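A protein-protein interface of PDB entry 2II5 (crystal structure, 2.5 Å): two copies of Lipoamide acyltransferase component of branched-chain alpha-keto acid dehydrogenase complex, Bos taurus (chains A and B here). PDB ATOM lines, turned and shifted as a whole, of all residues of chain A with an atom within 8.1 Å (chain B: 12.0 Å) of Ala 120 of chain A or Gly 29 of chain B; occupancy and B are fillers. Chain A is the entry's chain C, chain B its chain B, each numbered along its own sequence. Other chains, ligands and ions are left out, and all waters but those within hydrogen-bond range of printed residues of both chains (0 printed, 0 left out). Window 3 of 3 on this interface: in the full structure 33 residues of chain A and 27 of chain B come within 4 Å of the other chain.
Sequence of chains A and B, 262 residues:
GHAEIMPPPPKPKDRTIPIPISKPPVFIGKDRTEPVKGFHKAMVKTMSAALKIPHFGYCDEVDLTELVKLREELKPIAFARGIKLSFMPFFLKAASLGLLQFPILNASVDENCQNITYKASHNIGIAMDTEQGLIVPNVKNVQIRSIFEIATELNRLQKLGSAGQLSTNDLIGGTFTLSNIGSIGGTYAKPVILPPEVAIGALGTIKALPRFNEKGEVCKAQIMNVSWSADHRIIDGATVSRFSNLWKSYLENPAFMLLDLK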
ATOM      1  N   SER A  96     -12.605  23.831  19.755  1.00  0.00           N
ATOM      2  CA  SER A  96     -11.546  22.868  19.498  1.00  0.00           C
ATOM      3  C   SER A  96     -10.223  23.573  19.363  1.00  0.00           C
ATOM      4  O   SER A  96      -9.187  23.062  19.790  1.00  0.00           O
ATOM      5  CB  SER A  96     -11.794  22.148  18.185  1.00  0.00           C
ATOM      6  OG  SER A  96     -10.807  21.136  18.025  1.00  0.00           O
ATOM      7  N   LEU A  99      -9.061  24.393  22.803  1.00  0.00           N
ATOM      8  CA  LEU A  99      -8.753  23.168  23.555  1.00  0.00           C
ATOM      9  C   LEU A  99      -7.383  22.660  23.207  1.00  0.00           C
ATOM     10  O   LEU A  99      -6.705  22.063  24.034  1.00  0.00           O
ATOM     11  CB  LEU A  99      -9.766  22.084  23.294  1.00  0.00           C
ATOM     12  CG  LEU A  99     -10.967  21.658  24.168  1.00  0.00           C
ATOM     13  CD1 LEU A  99     -11.397  22.564  25.294  1.00  0.00           C
ATOM     14  CD2 LEU A  99     -12.146  21.325  23.272  1.00  0.00           C
ATOM     15  N   LEU A 100      -6.959  22.898  21.971  1.00  0.00           N
ATOM     16  CA  LEU A 100      -5.581  22.646  21.612  1.00  0.00           C
ATOM     17  C   LEU A 100      -4.599  23.405  22.540  1.00  0.00           C
ATOM     18  O   LEU A 100      -3.570  22.852  22.922  1.00  0.00           O
ATOM     19  CB  LEU A 100      -5.334  22.994  20.156  1.00  0.00           C
ATOM     20  CG  LEU A 100      -5.924  22.050  19.113  1.00  0.00           C
ATOM     21  CD1 LEU A 100      -5.670  22.674  17.708  1.00  0.00           C
ATOM     22  CD2 LEU A 100      -5.384  20.568  19.215  1.00  0.00           C
ATOM     23  N   PRO A 103      -5.520  21.876  26.855  1.00  0.00           N
ATOM     24  CA  PRO A 103      -6.016  20.529  26.747  1.00  0.00           C
ATOM     25  C   PRO A 103      -6.535  19.970  28.054  1.00  0.00           C
ATOM     26  O   PRO A 103      -7.291  19.008  28.045  1.00  0.00           O
ATOM     27  CB  PRO A 103      -4.786  19.741  26.236  1.00  0.00           C
ATOM     28  CG  PRO A 103      -3.612  20.523  26.746  1.00  0.00           C
ATOM     29  CD  PRO A 103      -4.067  21.943  26.560  1.00  0.00           C
ATOM     30  N   ASN A 106     -10.203  19.298  28.143  1.00  0.00           N
ATOM     31  CA  ASN A 106     -10.740  18.202  27.344  1.00  0.00           C
ATOM     32  C   ASN A 106     -10.256  16.918  27.960  1.00  0.00           C
ATOM     33  O   ASN A 106      -9.861  15.992  27.276  1.00  0.00           O
ATOM     34  CB  ASN A 106     -10.220  18.346  25.919  1.00  0.00           C
ATOM     35  CG  ASN A 106     -10.957  17.458  24.932  1.00  0.00           C
ATOM     36  OD1 ASN A 106     -12.133  17.651  24.673  1.00  0.00           O
ATOM     37  ND2 ASN A 106     -10.244  16.481  24.358  1.00  0.00           N
ATOM     38  N   ALA A 107     -10.258  16.866  29.273  1.00  0.00           N
ATOM     39  CA  ALA A 107      -9.632  15.801  30.025  1.00  0.00           C
ATOM     40  C   ALA A 107     -10.696  15.183  30.859  1.00  0.00           C
ATOM     41  O   ALA A 107     -11.788  15.700  30.953  1.00  0.00           O
ATOM     42  CB  ALA A 107      -8.564  16.390  30.948  1.00  0.00           C
ATOM     43  N   THR A 117      -6.858  12.036  32.874  1.00  0.00           N
ATOM     44  CA  THR A 117      -6.611  11.565  31.518  1.00  0.00           C
ATOM     45  C   THR A 117      -6.875  12.693  30.517  1.00  0.00           C
ATOM     46  O   THR A 117      -7.987  13.227  30.422  1.00  0.00           O
ATOM     47  CB  THR A 117      -7.457  10.334  31.193  1.00  0.00           C
ATOM     48  OG1 THR A 117      -7.137   9.322  32.140  1.00  0.00           O
ATOM     49  CG2 THR A 117      -7.202   9.787  29.725  1.00  0.00           C
ATOM     50  N   TYR A 118      -5.826  13.044  29.785  1.00  0.00           N
ATOM     51  CA  TYR A 118      -5.860  14.106  28.775  1.00  0.00           C
ATOM     52  C   TYR A 118      -6.266  13.417  27.505  1.00  0.00           C
ATOM     53  O   TYR A 118      -5.589  12.492  27.087  1.00  0.00           O
ATOM     54  CB  TYR A 118      -4.451  14.712  28.590  1.00  0.00           C
ATOM     55  CG  TYR A 118      -4.003  15.611  29.735  1.00  0.00           C
ATOM     56  CD1 TYR A 118      -3.539  15.066  30.930  1.00  0.00           C
ATOM     57  CD2 TYR A 118      -4.023  17.011  29.615  1.00  0.00           C
ATOM     58  CE1 TYR A 118      -3.135  15.877  31.967  1.00  0.00           C
ATOM     59  CE2 TYR A 118      -3.612  17.826  30.674  1.00  0.00           C
ATOM     60  CZ  TYR A 118      -3.183  17.245  31.843  1.00  0.00           C
ATOM     61  OH  TYR A 118      -2.757  18.010  32.908  1.00  0.00           O
ATOM     62  N   LYS A 119      -7.369  13.826  26.898  1.00  0.00           N
ATOM     63  CA  LYS A 119      -7.927  13.041  25.799  1.00  0.00           C
ATOM     64  C   LYS A 119      -7.611  13.672  24.446  1.00  0.00           C
ATOM     65  O   LYS A 119      -7.861  14.860  24.215  1.00  0.00           O
ATOM     66  CB  LYS A 119      -9.435  12.793  26.001  1.00  0.00           C
ATOM     67  CG  LYS A 119      -9.715  11.677  27.040  1.00  0.00           C
ATOM     68  CD  LYS A 119     -11.191  11.498  27.329  1.00  0.00           C
ATOM     69  CE  LYS A 119     -11.443  10.419  28.402  1.00  0.00           C
ATOM     70  NZ  LYS A 119     -12.882  10.371  28.909  1.00  0.00           N
ATOM     71  N   ALA A 120      -7.032  12.882  23.552  1.00  0.00           N
ATOM     72  CA  ALA A 120      -6.582  13.401  22.271  1.00  0.00           C
ATOM     73  C   ALA A 120      -7.746  13.949  21.429  1.00  0.00           C
ATOM     74  O   ALA A 120      -7.714  15.099  21.033  1.00  0.00           O
ATOM     75  CB  ALA A 120      -5.809  12.341  21.526  1.00  0.00           C
ATOM     76  N   SER A 121      -8.780  13.146  21.204  1.00  0.00           N
ATOM     77  CA  SER A 121      -9.859  13.495  20.311  1.00  0.00           C
ATOM     78  C   SER A 121     -10.722  14.579  20.911  1.00  0.00           C
ATOM     79  O   SER A 121     -10.950  14.620  22.144  1.00  0.00           O
ATOM     80  CB  SER A 121     -10.750  12.279  20.099  1.00  0.00           C
ATOM     81  OG  SER A 121     -10.064  11.280  19.394  1.00  0.00           O
ATOM     82  N   HIS A 122     -11.229  15.463  20.060  1.00  0.00           N
ATOM     83  CA  HIS A 122     -12.152  16.441  20.545  1.00  0.00           C
ATOM     84  C   HIS A 122     -13.534  15.962  20.149  1.00  0.00           C
ATOM     85  O   HIS A 122     -14.051  16.358  19.095  1.00  0.00           O
ATOM     86  CB  HIS A 122     -11.844  17.885  20.051  1.00  0.00           C
ATOM     87  CG  HIS A 122     -10.505  18.412  20.480  1.00  0.00           C
ATOM     88  ND1 HIS A 122      -9.977  19.595  19.989  1.00  0.00           N
ATOM     89  CD2 HIS A 122      -9.574  17.914  21.335  1.00  0.00           C
ATOM     90  CE1 HIS A 122      -8.790  19.804  20.524  1.00  0.00           C
ATOM     91  NE2 HIS A 122      -8.516  18.796  21.336  1.00  0.00           N
ATOM     92  N   ASN A 123     -14.117  15.118  21.000  1.00  0.00           N
ATOM     93  CA  ASN A 123     -15.477  14.674  20.824  1.00  0.00           C
ATOM     94  C   ASN A 123     -16.478  15.616  21.543  1.00  0.00           C
ATOM     95  O   ASN A 123     -16.774  15.452  22.747  1.00  0.00           O
ATOM     96  CB  ASN A 123     -15.596  13.221  21.301  1.00  0.00           C
ATOM     97  CG  ASN A 123     -14.663  12.244  20.524  1.00  0.00           C
ATOM     98  OD1 ASN A 123     -14.360  11.133  21.016  1.00  0.00           O
ATOM     99  ND2 ASN A 123     -14.239  12.638  19.310  1.00  0.00           N
ATOM    100  N   ASN A 141     -13.879  14.173  16.838  1.00  0.00           N
ATOM    101  CA  ASN A 141     -12.643  14.631  16.170  1.00  0.00           C
ATOM    102  C   ASN A 141     -12.750  16.013  15.469  1.00  0.00           C
ATOM    103  O   ASN A 141     -12.358  16.217  14.314  1.00  0.00           O
ATOM    104  CB  ASN A 141     -12.169  13.540  15.215  1.00  0.00           C
ATOM    105  CG  ASN A 141     -11.574  12.355  15.950  1.00  0.00           C
ATOM    106  OD1 ASN A 141     -10.906  12.507  16.971  1.00  0.00           O
ATOM    107  ND2 ASN A 141     -11.802  11.159  15.428  1.00  0.00           N
ATOM    108  N   VAL A 142     -13.303  16.957  16.206  1.00  0.00           N
ATOM    109  CA  VAL A 142     -13.533  18.271  15.693  1.00  0.00           C
ATOM    110  C   VAL A 142     -12.222  18.861  15.252  1.00  0.00           C
ATOM    111  O   VAL A 142     -12.167  19.628  14.311  1.00  0.00           O
ATOM    112  CB  VAL A 142     -14.296  19.119  16.724  1.00  0.00           C
ATOM    113  CG1 VAL A 142     -14.537  20.565  16.227  1.00  0.00           C
ATOM    114  CG2 VAL A 142     -15.640  18.441  17.017  1.00  0.00           C
ATOM    115  N   GLN A 143     -11.148  18.430  15.893  1.00  0.00           N
ATOM    116  CA  GLN A 143      -9.828  19.009  15.614  1.00  0.00           C
ATOM    117  C   GLN A 143      -9.342  18.707  14.190  1.00  0.00           C
ATOM    118  O   GLN A 143      -8.503  19.440  13.674  1.00  0.00           O
ATOM    119  CB  GLN A 143      -8.781  18.671  16.699  1.00  0.00           C
ATOM    120  CG  GLN A 143      -8.261  17.238  16.727  1.00  0.00           C
ATOM    121  CD  GLN A 143      -9.345  16.215  17.068  1.00  0.00           C
ATOM    122  OE1 GLN A 143     -10.450  16.564  17.512  1.00  0.00           O
ATOM    123  NE2 GLN A 143      -9.034  14.934  16.849  1.00  0.00           N
ATOM    124  N   THR A 175     -15.956  14.176  25.047  1.00  0.00           N
ATOM    125  CA  THR A 175     -14.906  14.717  25.899  1.00  0.00           C
ATOM    126  C   THR A 175     -15.222  16.110  26.468  1.00  0.00           C
ATOM    127  O   THR A 175     -14.593  16.538  27.431  1.00  0.00           O
ATOM    128  CB  THR A 175     -13.602  14.815  25.144  1.00  0.00           C
ATOM    129  OG1 THR A 175     -13.794  15.668  24.006  1.00  0.00           O
ATOM    130  CG2 THR A 175     -13.099  13.406  24.699  1.00  0.00           C
ATOM    131  N   GLY B  29      -1.314  12.865  20.746  1.00  0.00           N
ATOM    132  CA  GLY B  29      -1.778  11.902  19.692  1.00  0.00           C
ATOM    133  C   GLY B  29      -2.611  10.749  20.231  1.00  0.00           C
ATOM    134  O   GLY B  29      -3.556  10.296  19.570  1.00  0.00           O
ATOM    135  N   LYS B  30      -2.238  10.271  21.425  1.00  0.00           N
ATOM    136  CA  LYS B  30      -2.956   9.223  22.172  1.00  0.00           C
ATOM    137  C   LYS B  30      -3.363   9.795  23.545  1.00  0.00           C
ATOM    138  O   LYS B  30      -2.912  10.873  23.938  1.00  0.00           O
ATOM    139  CB  LYS B  30      -2.065   7.983  22.356  1.00  0.00           C
ATOM    140  CG  LYS B  30      -1.441   7.425  21.067  1.00  0.00           C
ATOM    141  CD  LYS B  30      -2.320   6.329  20.459  1.00  0.00           C
ATOM    142  CE  LYS B  30      -2.200   6.255  18.908  1.00  0.00           C
ATOM    143  NZ  LYS B  30      -0.997   5.504  18.387  1.00  0.00           N
ATOM    144  N   ASP B  31      -4.207   9.084  24.283  1.00  0.00           N
ATOM    145  CA  ASP B  31      -4.598   9.553  25.595  1.00  0.00           C
ATOM    146  C   ASP B  31      -3.494   9.362  26.635  1.00  0.00           C
ATOM    147  O   ASP B  31      -2.948   8.273  26.774  1.00  0.00           O
ATOM    148  CB  ASP B  31      -5.860   8.831  26.037  1.00  0.00           C
ATOM    149  CG  ASP B  31      -7.082   9.282  25.285  1.00  0.00           C
ATOM    150  OD1 ASP B  31      -6.985  10.202  24.446  1.00  0.00           O
ATOM    151  OD2 ASP B  31      -8.148   8.697  25.529  1.00  0.00           O
ATOM    152  N   ARG B  32      -3.180  10.426  27.363  1.00  0.00           N
ATOM    153  CA  ARG B  32      -2.174  10.408  28.415  1.00  0.00           C
ATOM    154  C   ARG B  32      -2.888  10.375  29.790  1.00  0.00           C
ATOM    155  O   ARG B  32      -3.791  11.174  30.020  1.00  0.00           O
ATOM    156  CB  ARG B  32      -1.336  11.693  28.277  1.00  0.00           C
ATOM    157  CG  ARG B  32       0.136  11.603  28.645  1.00  0.00           C
ATOM    158  CD  ARG B  32       0.878  12.945  28.365  1.00  0.00           C
ATOM    159  NE  ARG B  32       0.937  13.849  29.537  1.00  0.00           N
ATOM    160  CZ  ARG B  32       0.567  15.146  29.547  1.00  0.00           C
ATOM    161  NH1 ARG B  32       0.103  15.748  28.447  1.00  0.00           N
ATOM    162  NH2 ARG B  32       0.651  15.857  30.671  1.00  0.00           N
ATOM    163  N   THR B  33      -2.512   9.463  30.693  1.00  0.00           N
ATOM    164  CA  THR B  33      -3.018   9.520  32.087  1.00  0.00           C
ATOM    165  C   THR B  33      -1.957   9.922  33.093  1.00  0.00           C
ATOM    166  O   THR B  33      -0.801   9.509  32.991  1.00  0.00           O
ATOM    167  CB  THR B  33      -3.654   8.218  32.551  1.00  0.00           C
ATOM    168  OG1 THR B  33      -4.676   7.856  31.626  1.00  0.00           O
ATOM    169  CG2 THR B  33      -4.288   8.390  33.930  1.00  0.00           C
ATOM    170  N   GLU B  34      -2.341  10.735  34.066  1.00  0.00           N
ATOM    171  CA  GLU B  34      -1.366  11.261  35.007  1.00  0.00           C
ATOM    172  C   GLU B  34      -1.879  11.394  36.432  1.00  0.00           C
ATOM    173  O   GLU B  34      -3.064  11.708  36.651  1.00  0.00           O
ATOM    174  CB  GLU B  34      -0.864  12.608  34.528  1.00  0.00           C
ATOM    175  CG  GLU B  34      -0.207  12.470  33.198  1.00  0.00           C
ATOM    176  CD  GLU B  34       0.681  13.624  32.849  1.00  0.00           C
ATOM    177  OE1 GLU B  34       0.446  14.735  33.402  1.00  0.00           O
ATOM    178  OE2 GLU B  34       1.595  13.397  32.007  1.00  0.00           O
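OG1 of Thr 117 of chain A sits at hydrogen-bond distance from OG1 of Thr 33 of chain B, 2.9 Å away. O of Arg 32 of chain B lies within hydrogen-bond range of N of Tyr 118 of chain A (2.8 Å). The backbone NH (N) of Ala 120 of chain A is in hydrogen-bond range of the side-chain carboxylate (OD1) of Asp 31 of chain B (2.8 Å).
The side-chain amide nitrogen (ND2) of Asn 106 of chain A is in hydrogen-bond range of the backbone carbonyl oxygen (O) of Lys 119 of chain A. The guanidinium group (NE) of Arg 32 of chain B is in salt-bridge range of the side-chain carboxylate (OE2) of Glu 34 of chain B (2.6 Å).
CA of Thr 117 of chain A touches O of Arg 32 of chain B, 3.2 Å away. CA of Asp 31 of chain B touches O of Tyr 118 of chain A, at 3.4 Å. CA of Lys 119 of chain A touches OD1 of Asp 31 of chain B (3.3 Å). Gly 29 of chain B touches Ala 120 of chain A.
Ala 120 of chain A touches just these residues of chain B: Gly 29 (3.6 Å) and Asp 31 (2.8 Å). No residue of chain B comes within 4 Å of Ser 121 of chain A. No residue of chain B comes within 4 Å of His 122 of chain A. Of the printed residues of chain A, Thr 33 of chain B touches Thr 117 (2.9 Å). Of the printed residues of chain A, Asp 31 of chain B touches Tyr 118 (3.4 Å), Lys 119 (3.3 Å) and Ala 120 (2.8 Å). Of the printed residues of chain A, Arg 32 of chain B touches Thr 117 and Tyr 118. The nearest residue of chain A that does not touch Gly 29 of chain B is Ser 121 of chain A (6.2 Å).
Of the 17 printed residues of chain A, 4 touch a printed residue of chain B. Hydrophobic or aromatic side chains of chain A within 4 Å of the printed part of chain B: Tyr 118 and Ala 120. Among the printed residues, 7 pairs touch across the chains. Among the printed residues, no Asp or Glu carboxylate lies within 4 Å of a Lys or Arg side-chain nitrogen of the other chain.
No position is printed for both chains. Of the 7 pairs that touch across the chains among the printed residues, none has its exchanged pair printed and touching as well.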
